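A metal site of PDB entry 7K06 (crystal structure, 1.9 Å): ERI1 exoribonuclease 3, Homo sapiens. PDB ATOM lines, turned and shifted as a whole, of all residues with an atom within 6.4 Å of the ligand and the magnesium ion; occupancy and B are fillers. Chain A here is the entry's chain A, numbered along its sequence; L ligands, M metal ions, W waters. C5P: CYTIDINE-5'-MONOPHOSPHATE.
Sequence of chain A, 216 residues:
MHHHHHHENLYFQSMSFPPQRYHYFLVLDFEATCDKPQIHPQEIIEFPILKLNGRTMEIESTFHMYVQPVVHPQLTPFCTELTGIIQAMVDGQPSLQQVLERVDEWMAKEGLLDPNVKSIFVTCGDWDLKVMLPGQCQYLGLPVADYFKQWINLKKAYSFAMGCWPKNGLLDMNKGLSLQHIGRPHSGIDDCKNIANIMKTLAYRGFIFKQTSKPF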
ATOM      1  N   ASP A  29       0.709   9.441  15.154  1.00  0.00           N
ATOM      2  CA  ASP A  29       0.164   8.090  15.286  1.00  0.00           C
ATOM      3  C   ASP A  29       1.340   7.122  15.428  1.00  0.00           C
ATOM      4  O   ASP A  29       1.959   6.757  14.428  1.00  0.00           O
ATOM      5  CB  ASP A  29      -0.698   7.730  14.086  1.00  0.00           C
ATOM      6  CG  ASP A  29      -1.616   6.549  14.363  1.00  0.00           C
ATOM      7  OD1 ASP A  29      -2.828   6.769  14.592  1.00  0.00           O
ATOM      8  OD2 ASP A  29      -1.128   5.402  14.356  1.00  0.00           O
ATOM      9  N   PHE A  30       1.633   6.715  16.657  1.00  0.00           N
ATOM     10  CA  PHE A  30       2.740   5.802  16.903  1.00  0.00           C
ATOM     11  C   PHE A  30       2.455   4.422  16.339  1.00  0.00           C
ATOM     12  O   PHE A  30       1.294   4.003  16.218  1.00  0.00           O
ATOM     13  CB  PHE A  30       3.003   5.664  18.402  1.00  0.00           C
ATOM     14  CG  PHE A  30       3.517   6.905  19.064  1.00  0.00           C
ATOM     15  CD1 PHE A  30       4.544   7.645  18.508  1.00  0.00           C
ATOM     16  CD2 PHE A  30       2.958   7.325  20.265  1.00  0.00           C
ATOM     17  CE1 PHE A  30       5.010   8.787  19.139  1.00  0.00           C
ATOM     18  CE2 PHE A  30       3.424   8.467  20.896  1.00  0.00           C
ATOM     19  CZ  PHE A  30       4.447   9.198  20.330  1.00  0.00           C
ATOM     20  N   GLU A  31       3.517   3.698  16.009  1.00  0.00           N
ATOM     21  CA  GLU A  31       3.503   2.249  15.997  1.00  0.00           C
ATOM     22  C   GLU A  31       4.497   1.772  17.037  1.00  0.00           C
ATOM     23  O   GLU A  31       5.507   2.433  17.291  1.00  0.00           O
ATOM     24  CB  GLU A  31       3.844   1.671  14.621  1.00  0.00           C
ATOM     25  CG  GLU A  31       2.931   2.155  13.496  1.00  0.00           C
ATOM     26  CD  GLU A  31       1.466   1.839  13.733  1.00  0.00           C
ATOM     27  OE1 GLU A  31       1.149   0.836  14.409  1.00  0.00           O
ATOM     28  OE2 GLU A  31       0.627   2.608  13.222  1.00  0.00           O
ATOM     29  N   ALA A  32       4.201   0.628  17.664  1.00  0.00           N
ATOM     30  CA  ALA A  32       5.007   0.135  18.769  1.00  0.00           C
ATOM     31  C   ALA A  32       5.235  -1.360  18.601  1.00  0.00           C
ATOM     32  O   ALA A  32       4.476  -2.048  17.921  1.00  0.00           O
ATOM     33  CB  ALA A  32       4.328   0.404  20.127  1.00  0.00           C
ATOM     34  N   THR A  33       6.308  -1.851  19.236  1.00  0.00           N
ATOM     35  CA  THR A  33       6.509  -3.293  19.334  1.00  0.00           C
ATOM     36  C   THR A  33       5.264  -3.953  19.906  1.00  0.00           C
ATOM     37  O   THR A  33       4.554  -3.380  20.742  1.00  0.00           O
ATOM     38  CB  THR A  33       7.703  -3.626  20.231  1.00  0.00           C
ATOM     39  OG1 THR A  33       7.489  -3.081  21.545  1.00  0.00           O
ATOM     40  CG2 THR A  33       9.009  -3.065  19.645  1.00  0.00           C
ATOM     41  N   CYS A  34       4.986  -5.167  19.465  1.00  0.00           N
ATOM     42  CA  CYS A  34       3.783  -5.858  19.875  1.00  0.00           C
ATOM     43  C   CYS A  34       3.976  -7.355  19.656  1.00  0.00           C
ATOM     44  O   CYS A  34       4.989  -7.798  19.109  1.00  0.00           O
ATOM     45  CB  CYS A  34       2.565  -5.329  19.119  1.00  0.00           C
ATOM     46  SG  CYS A  34       2.808  -5.260  17.344  1.00  0.00           S
ATOM     47  N   ASP A  35       2.974  -8.125  20.097  1.00  0.00           N
ATOM     48  CA  ASP A  35       2.942  -9.572  19.944  1.00  0.00           C
ATOM     49  C   ASP A  35       1.544 -10.032  20.331  1.00  0.00           C
ATOM     50  O   ASP A  35       0.693  -9.226  20.737  1.00  0.00           O
ATOM     51  CB  ASP A  35       4.025 -10.246  20.802  1.00  0.00           C
ATOM     52  CG  ASP A  35       4.441 -11.606  20.258  1.00  0.00           C
ATOM     53  OD1 ASP A  35       3.859 -12.059  19.251  1.00  0.00           O
ATOM     54  OD2 ASP A  35       5.369 -12.211  20.833  1.00  0.00           O
ATOM     55  N   LYS A  36       1.309 -11.338  20.215  1.00  0.00           N
ATOM     56  CA  LYS A  36       0.080 -11.963  20.701  1.00  0.00           C
ATOM     57  C   LYS A  36       0.474 -13.202  21.483  1.00  0.00           C
ATOM     58  O   LYS A  36       1.010 -14.154  20.889  1.00  0.00           O
ATOM     59  CB  LYS A  36      -0.870 -12.297  19.552  1.00  0.00           C
ATOM     60  CG  LYS A  36      -1.483 -11.068  18.884  1.00  0.00           C
ATOM     61  CD  LYS A  36      -2.451 -10.348  19.827  1.00  0.00           C
ATOM     62  CE  LYS A  36      -2.876  -8.984  19.290  1.00  0.00           C
ATOM     63  NZ  LYS A  36      -1.899  -7.898  19.613  1.00  0.00           N
ATOM     64  N   GLN A  38       0.153  -9.804  24.164  1.00  0.00           N
ATOM     65  CA  GLN A  38       0.844  -8.537  23.974  1.00  0.00           C
ATOM     66  C   GLN A  38       2.210  -8.540  24.644  1.00  0.00           C
ATOM     67  O   GLN A  38       2.388  -9.055  25.753  1.00  0.00           O
ATOM     68  CB  GLN A  38      -0.016  -7.389  24.516  1.00  0.00           C
ATOM     69  CG  GLN A  38       0.484  -6.009  24.143  1.00  0.00           C
ATOM     70  CD  GLN A  38       0.738  -5.871  22.652  1.00  0.00           C
ATOM     71  OE1 GLN A  38       1.786  -6.281  22.159  1.00  0.00           O
ATOM     72  NE2 GLN A  38      -0.221  -5.301  21.932  1.00  0.00           N
ATOM     73  N   GLN A  42       5.770  -2.425  25.785  1.00  0.00           N
ATOM     74  CA  GLN A  42       5.781  -1.967  24.414  1.00  0.00           C
ATOM     75  C   GLN A  42       6.743  -0.798  24.266  1.00  0.00           C
ATOM     76  O   GLN A  42       7.002  -0.064  25.228  1.00  0.00           O
ATOM     77  CB  GLN A  42       4.384  -1.539  23.970  1.00  0.00           C
ATOM     78  CG  GLN A  42       3.397  -2.690  23.827  1.00  0.00           C
ATOM     79  CD  GLN A  42       2.076  -2.234  23.231  1.00  0.00           C
ATOM     80  OE1 GLN A  42       1.147  -1.886  23.959  1.00  0.00           O
ATOM     81  NE2 GLN A  42       1.996  -2.208  21.908  1.00  0.00           N
ATOM     82  N   ILE A  45       8.255   2.333  17.882  1.00  0.00           N
ATOM     83  CA  ILE A  45       9.148   2.026  16.759  1.00  0.00           C
ATOM     84  C   ILE A  45       8.927   2.907  15.535  1.00  0.00           C
ATOM     85  O   ILE A  45       9.749   2.867  14.626  1.00  0.00           O
ATOM     86  CB  ILE A  45       9.061   0.536  16.342  1.00  0.00           C
ATOM     87  CG1 ILE A  45       7.656   0.166  15.901  1.00  0.00           C
ATOM     88  CG2 ILE A  45       9.558  -0.358  17.464  1.00  0.00           C
ATOM     89  CD1 ILE A  45       7.540  -1.254  15.389  1.00  0.00           C
ATOM     90  N   PHE A  78       4.486 -11.118  14.439  1.00  0.00           N
ATOM     91  CA  PHE A  78       3.225 -10.389  14.513  1.00  0.00           C
ATOM     92  C   PHE A  78       3.440  -8.900  14.274  1.00  0.00           C
ATOM     93  O   PHE A  78       2.699  -8.266  13.504  1.00  0.00           O
ATOM     94  CB  PHE A  78       2.546 -10.618  15.863  1.00  0.00           C
ATOM     95  CG  PHE A  78       1.304  -9.800  16.040  1.00  0.00           C
ATOM     96  CD1 PHE A  78       0.106 -10.227  15.509  1.00  0.00           C
ATOM     97  CD2 PHE A  78       1.352  -8.589  16.695  1.00  0.00           C
ATOM     98  CE1 PHE A  78      -1.033  -9.467  15.646  1.00  0.00           C
ATOM     99  CE2 PHE A  78       0.217  -7.815  16.830  1.00  0.00           C
ATOM    100  CZ  PHE A  78      -0.978  -8.256  16.308  1.00  0.00           C
ATOM    101  N   CYS A  79       4.445  -8.322  14.919  1.00  0.00           N
ATOM    102  CA  CYS A  79       4.685  -6.888  14.794  1.00  0.00           C
ATOM    103  C   CYS A  79       4.977  -6.498  13.356  1.00  0.00           C
ATOM    104  O   CYS A  79       4.423  -5.523  12.838  1.00  0.00           O
ATOM    105  CB  CYS A  79       5.840  -6.473  15.705  1.00  0.00           C
ATOM    106  SG  CYS A  79       6.354  -4.756  15.503  1.00  0.00           S
ATOM    107  N   LEU A  82       1.768  -6.885  11.351  1.00  0.00           N
ATOM    108  CA  LEU A  82       0.766  -5.870  11.641  1.00  0.00           C
ATOM    109  C   LEU A  82       1.131  -4.534  11.014  1.00  0.00           C
ATOM    110  O   LEU A  82       0.319  -3.912  10.318  1.00  0.00           O
ATOM    111  CB  LEU A  82       0.598  -5.709  13.152  1.00  0.00           C
ATOM    112  CG  LEU A  82      -0.442  -4.667  13.557  1.00  0.00           C
ATOM    113  CD1 LEU A  82      -1.851  -5.184  13.253  1.00  0.00           C
ATOM    114  CD2 LEU A  82      -0.288  -4.303  15.036  1.00  0.00           C
ATOM    115  N   THR A  83       2.364  -4.066  11.266  1.00  0.00           N
ATOM    116  CA  THR A  83       2.777  -2.720  10.893  1.00  0.00           C
ATOM    117  C   THR A  83       3.481  -2.649   9.549  1.00  0.00           C
ATOM    118  O   THR A  83       3.597  -1.554   8.990  1.00  0.00           O
ATOM    119  CB  THR A  83       3.732  -2.157  11.954  1.00  0.00           C
ATOM    120  OG1 THR A  83       4.945  -2.910  11.942  1.00  0.00           O
ATOM    121  CG2 THR A  83       3.101  -2.234  13.337  1.00  0.00           C
ATOM    122  N   TRP A 127      -4.602   6.808  23.258  1.00  0.00           N
ATOM    123  CA  TRP A 127      -3.559   5.875  23.672  1.00  0.00           C
ATOM    124  C   TRP A 127      -2.162   6.461  23.485  1.00  0.00           C
ATOM    125  O   TRP A 127      -1.296   6.312  24.365  1.00  0.00           O
ATOM    126  CB  TRP A 127      -3.698   4.576  22.889  1.00  0.00           C
ATOM    127  CG  TRP A 127      -2.620   3.571  23.188  1.00  0.00           C
ATOM    128  CD1 TRP A 127      -2.545   2.764  24.281  1.00  0.00           C
ATOM    129  CD2 TRP A 127      -1.485   3.251  22.377  1.00  0.00           C
ATOM    130  NE1 TRP A 127      -1.417   1.978  24.210  1.00  0.00           N
ATOM    131  CE2 TRP A 127      -0.755   2.259  23.043  1.00  0.00           C
ATOM    132  CE3 TRP A 127      -1.015   3.727  21.136  1.00  0.00           C
ATOM    133  CZ2 TRP A 127       0.414   1.714  22.528  1.00  0.00           C
ATOM    134  CZ3 TRP A 127       0.152   3.186  20.637  1.00  0.00           C
ATOM    135  CH2 TRP A 127       0.853   2.192  21.319  1.00  0.00           C
ATOM    136  N   ASP A 128      -1.927   7.141  22.362  1.00  0.00           N
ATOM    137  CA  ASP A 128      -0.573   7.537  22.002  1.00  0.00           C
ATOM    138  C   ASP A 128       0.056   8.444  23.053  1.00  0.00           C
ATOM    139  O   ASP A 128       1.179   8.217  23.498  1.00  0.00           O
ATOM    140  CB  ASP A 128      -0.582   8.225  20.642  1.00  0.00           C
ATOM    141  CG  ASP A 128      -1.165   7.337  19.572  1.00  0.00           C
ATOM    142  OD1 ASP A 128      -0.388   6.821  18.745  1.00  0.00           O
ATOM    143  OD2 ASP A 128      -2.402   7.127  19.577  1.00  0.00           O
ATOM    144  N   LEU A 170     -10.185   4.807  12.524  1.00  0.00           N
ATOM    145  CA  LEU A 170     -10.053   5.502  11.248  1.00  0.00           C
ATOM    146  C   LEU A 170     -10.896   4.846  10.165  1.00  0.00           C
ATOM    147  O   LEU A 170     -11.445   5.540   9.300  1.00  0.00           O
ATOM    148  CB  LEU A 170      -8.588   5.548  10.817  1.00  0.00           C
ATOM    149  CG  LEU A 170      -7.624   6.298  11.722  1.00  0.00           C
ATOM    150  CD1 LEU A 170      -6.200   6.194  11.191  1.00  0.00           C
ATOM    151  CD2 LEU A 170      -8.064   7.738  11.861  1.00  0.00           C
ATOM    152  N   PRO A 185      -3.214   0.423   6.555  1.00  0.00           N
ATOM    153  CA  PRO A 185      -3.541   0.498   7.979  1.00  0.00           C
ATOM    154  C   PRO A 185      -2.388   0.011   8.850  1.00  0.00           C
ATOM    155  O   PRO A 185      -1.650  -0.898   8.469  1.00  0.00           O
ATOM    156  CB  PRO A 185      -4.770  -0.413   8.124  1.00  0.00           C
ATOM    157  CG  PRO A 185      -5.378  -0.426   6.743  1.00  0.00           C
ATOM    158  CD  PRO A 185      -4.206  -0.377   5.806  1.00  0.00           C
ATOM    159  N   HIS A 186      -2.232   0.638  10.014  1.00  0.00           N
ATOM    160  CA  HIS A 186      -1.190   0.354  11.003  1.00  0.00           C
ATOM    161  C   HIS A 186       0.204   0.751  10.514  1.00  0.00           C
ATOM    162  O   HIS A 186       1.203   0.355  11.133  1.00  0.00           O
ATOM    163  CB  HIS A 186      -1.205  -1.110  11.442  1.00  0.00           C
ATOM    164  CG  HIS A 186      -2.551  -1.605  11.844  1.00  0.00           C
ATOM    165  ND1 HIS A 186      -3.142  -1.259  13.044  1.00  0.00           N
ATOM    166  CD2 HIS A 186      -3.439  -2.395  11.204  1.00  0.00           C
ATOM    167  CE1 HIS A 186      -4.339  -1.823  13.124  1.00  0.00           C
ATOM    168  NE2 HIS A 186      -4.536  -2.526  12.027  1.00  0.00           N
ATOM    169  N   SER A 187       0.300   1.486   9.410  1.00  0.00           N
ATOM    170  CA  SER A 187       1.497   2.249   9.099  1.00  0.00           C
ATOM    171  C   SER A 187       1.325   3.613   9.750  1.00  0.00           C
ATOM    172  O   SER A 187       0.326   4.293   9.502  1.00  0.00           O
ATOM    173  CB  SER A 187       1.700   2.390   7.589  1.00  0.00           C
ATOM    174  OG  SER A 187       2.609   3.433   7.297  1.00  0.00           O
ATOM    175  N   GLY A 188       2.278   3.999  10.595  1.00  0.00           N
ATOM    176  CA  GLY A 188       2.130   5.253  11.327  1.00  0.00           C
ATOM    177  C   GLY A 188       1.913   6.441  10.414  1.00  0.00           C
ATOM    178  O   GLY A 188       0.968   7.209  10.581  1.00  0.00           O
ATOM    179  N   ASP A 191      -1.456   6.199   8.691  1.00  0.00           N
ATOM    180  CA  ASP A 191      -2.526   6.536   9.624  1.00  0.00           C
ATOM    181  C   ASP A 191      -2.615   8.056   9.793  1.00  0.00           C
ATOM    182  O   ASP A 191      -3.723   8.612   9.853  1.00  0.00           O
ATOM    183  CB  ASP A 191      -2.286   5.856  10.974  1.00  0.00           C
ATOM    184  CG  ASP A 191      -2.616   4.366  10.943  1.00  0.00           C
ATOM    185  OD1 ASP A 191      -3.250   3.913   9.961  1.00  0.00           O
ATOM    186  OD2 ASP A 191      -2.249   3.660  11.896  1.00  0.00           O
HETATM  187  O3P C5P L   1      -3.827   0.854  15.295  1.00  0.00           O
HETATM  188  P   C5P L   1      -2.385   1.193  15.477  1.00  0.00           P
HETATM  189  O1P C5P L   1      -2.115   2.652  15.583  1.00  0.00           O
HETATM  190  O2P C5P L   1      -1.475   0.567  14.472  1.00  0.00           O
HETATM  191  O5' C5P L   1      -2.077   0.580  16.935  1.00  0.00           O
HETATM  192  C5' C5P L   1      -0.978   1.026  17.747  1.00  0.00           C
HETATM  193  C4' C5P L   1      -0.137  -0.133  18.255  1.00  0.00           C
HETATM  194  O4' C5P L   1      -0.944  -1.024  19.062  1.00  0.00           O
HETATM  195  C3' C5P L   1       0.516  -1.040  17.207  1.00  0.00           C
HETATM  196  O3' C5P L   1       1.742  -0.521  16.715  1.00  0.00           O
HETATM  197  C2' C5P L   1       0.700  -2.342  17.987  1.00  0.00           C
HETATM  198  O2' C5P L   1       1.851  -2.227  18.820  1.00  0.00           O
HETATM  199  C1' C5P L   1      -0.534  -2.368  18.875  1.00  0.00           C
HETATM  200  N1  C5P L   1      -1.599  -3.210  18.257  1.00  0.00           N
HETATM  201  C2  C5P L   1      -1.538  -4.578  18.507  1.00  0.00           C
HETATM  202  N3  C5P L   1      -2.484  -5.349  17.958  1.00  0.00           N
HETATM  203  C4  C5P L   1      -3.468  -4.884  17.212  1.00  0.00           C
HETATM  204  C5  C5P L   1      -3.556  -3.465  16.952  1.00  0.00           C
HETATM  205  C6  C5P L   1      -2.620  -2.680  17.483  1.00  0.00           C
HETATM  206  O2  C5P L   1      -0.625  -4.988  19.200  1.00  0.00           O
HETATM  207  N4  C5P L   1      -4.368  -5.725  16.713  1.00  0.00           N
HETATM  208 MG    MG M   1      -1.125   3.528  13.828  1.00  0.00          MG
HETATM  209  O   HOH W   1      -4.038   0.683  18.451  1.00  0.00           O
HETATM  210  O   HOH W   2      -4.222   2.191  12.851  1.00  0.00           O
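The side-chain amide nitrogen (NE2) of Gln 38 sits at hydrogen-bond distance from an oxygen (O2) of the ligand (2.8 Å). N of Ala 32 lies within hydrogen-bond range of O3' of the ligand (2.9 Å). O of Ala 32 lies within hydrogen-bond range of O2' of the ligand (2.8 Å). A ring nitrogen (ND1) of His 186 is in hydrogen-bond range of an oxygen (O2P) of the ligand (2.9 Å). An oxygen (O2') of the ligand sits at hydrogen-bond distance from the side-chain amide nitrogen (NE2) of Gln 42. The side-chain amino group (NZ) of Lys 36 sits at hydrogen-bond distance from a nitrogen (N3) of the ligand (3.1 Å). SG of Cys 34 sits close to O2' of the ligand (3.5 Å).
The side-chain carboxylate (OE2) of Glu 31 sits close to the backbone NH (N) of Gly 188. The backbone carbonyl oxygen of Glu 31 is in hydrogen-bond range of the backbone NH of Ile 45 (2.8 Å). The backbone NH (N) of His 186 is in hydrogen-bond range of the side-chain carboxylate (OD1) of Asp 191 (3.4 Å). The side-chain amide oxygen of Gln 38 lies within hydrogen-bond range of the backbone NH of Asp 35 (3.0 Å). The backbone carbonyl oxygen (O) of Ala 32 is in hydrogen-bond range of the side-chain sulfur (SG) of Cys 34. NE2 of Gln 42 lies within hydrogen-bond range of O of Thr 33 (3.0 Å). The side-chain carboxylate of Asp 128 is in hydrogen-bond range of the backbone NH of Phe 30 (2.9 Å).
Merely in contact with the ligand: Phe 30 (3.7 Å), Thr 33 (3.5 Å), Phe 78 (3.7 Å), Leu 82 (3.6 Å) and Trp 127 (3.8 Å). Hydrophobic or aromatic side chains within 4 Å of the ligand: Ala 32, Phe 78, Leu 82, Trp 127 and His 186. Within 4 Å of the ligand: Asp 29, Phe 30, Glu 31, Ala 32, Thr 33, Cys 34, Lys 36, Gln 38, Gln 42, Phe 78, Leu 82, Trp 127, His 186 and Asp 191.
Merely in contact with the magnesium ion: Phe 30 (3.4 Å). Of the 23 residues printed, 4 come within 4 Å of the magnesium ion. Along chain A the residues within 4 Å of the magnesium ion span positions 29 to 191.
The magnesium ion is bound by the side-chain carboxylate of Asp 29 (1.9 Å), the side-chain carboxylate of Glu 31 (2.1 Å), an oxygen (O1P) of the ligand (2.2 Å) and the side-chain carboxylate of Asp 191 (2.2 Å).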
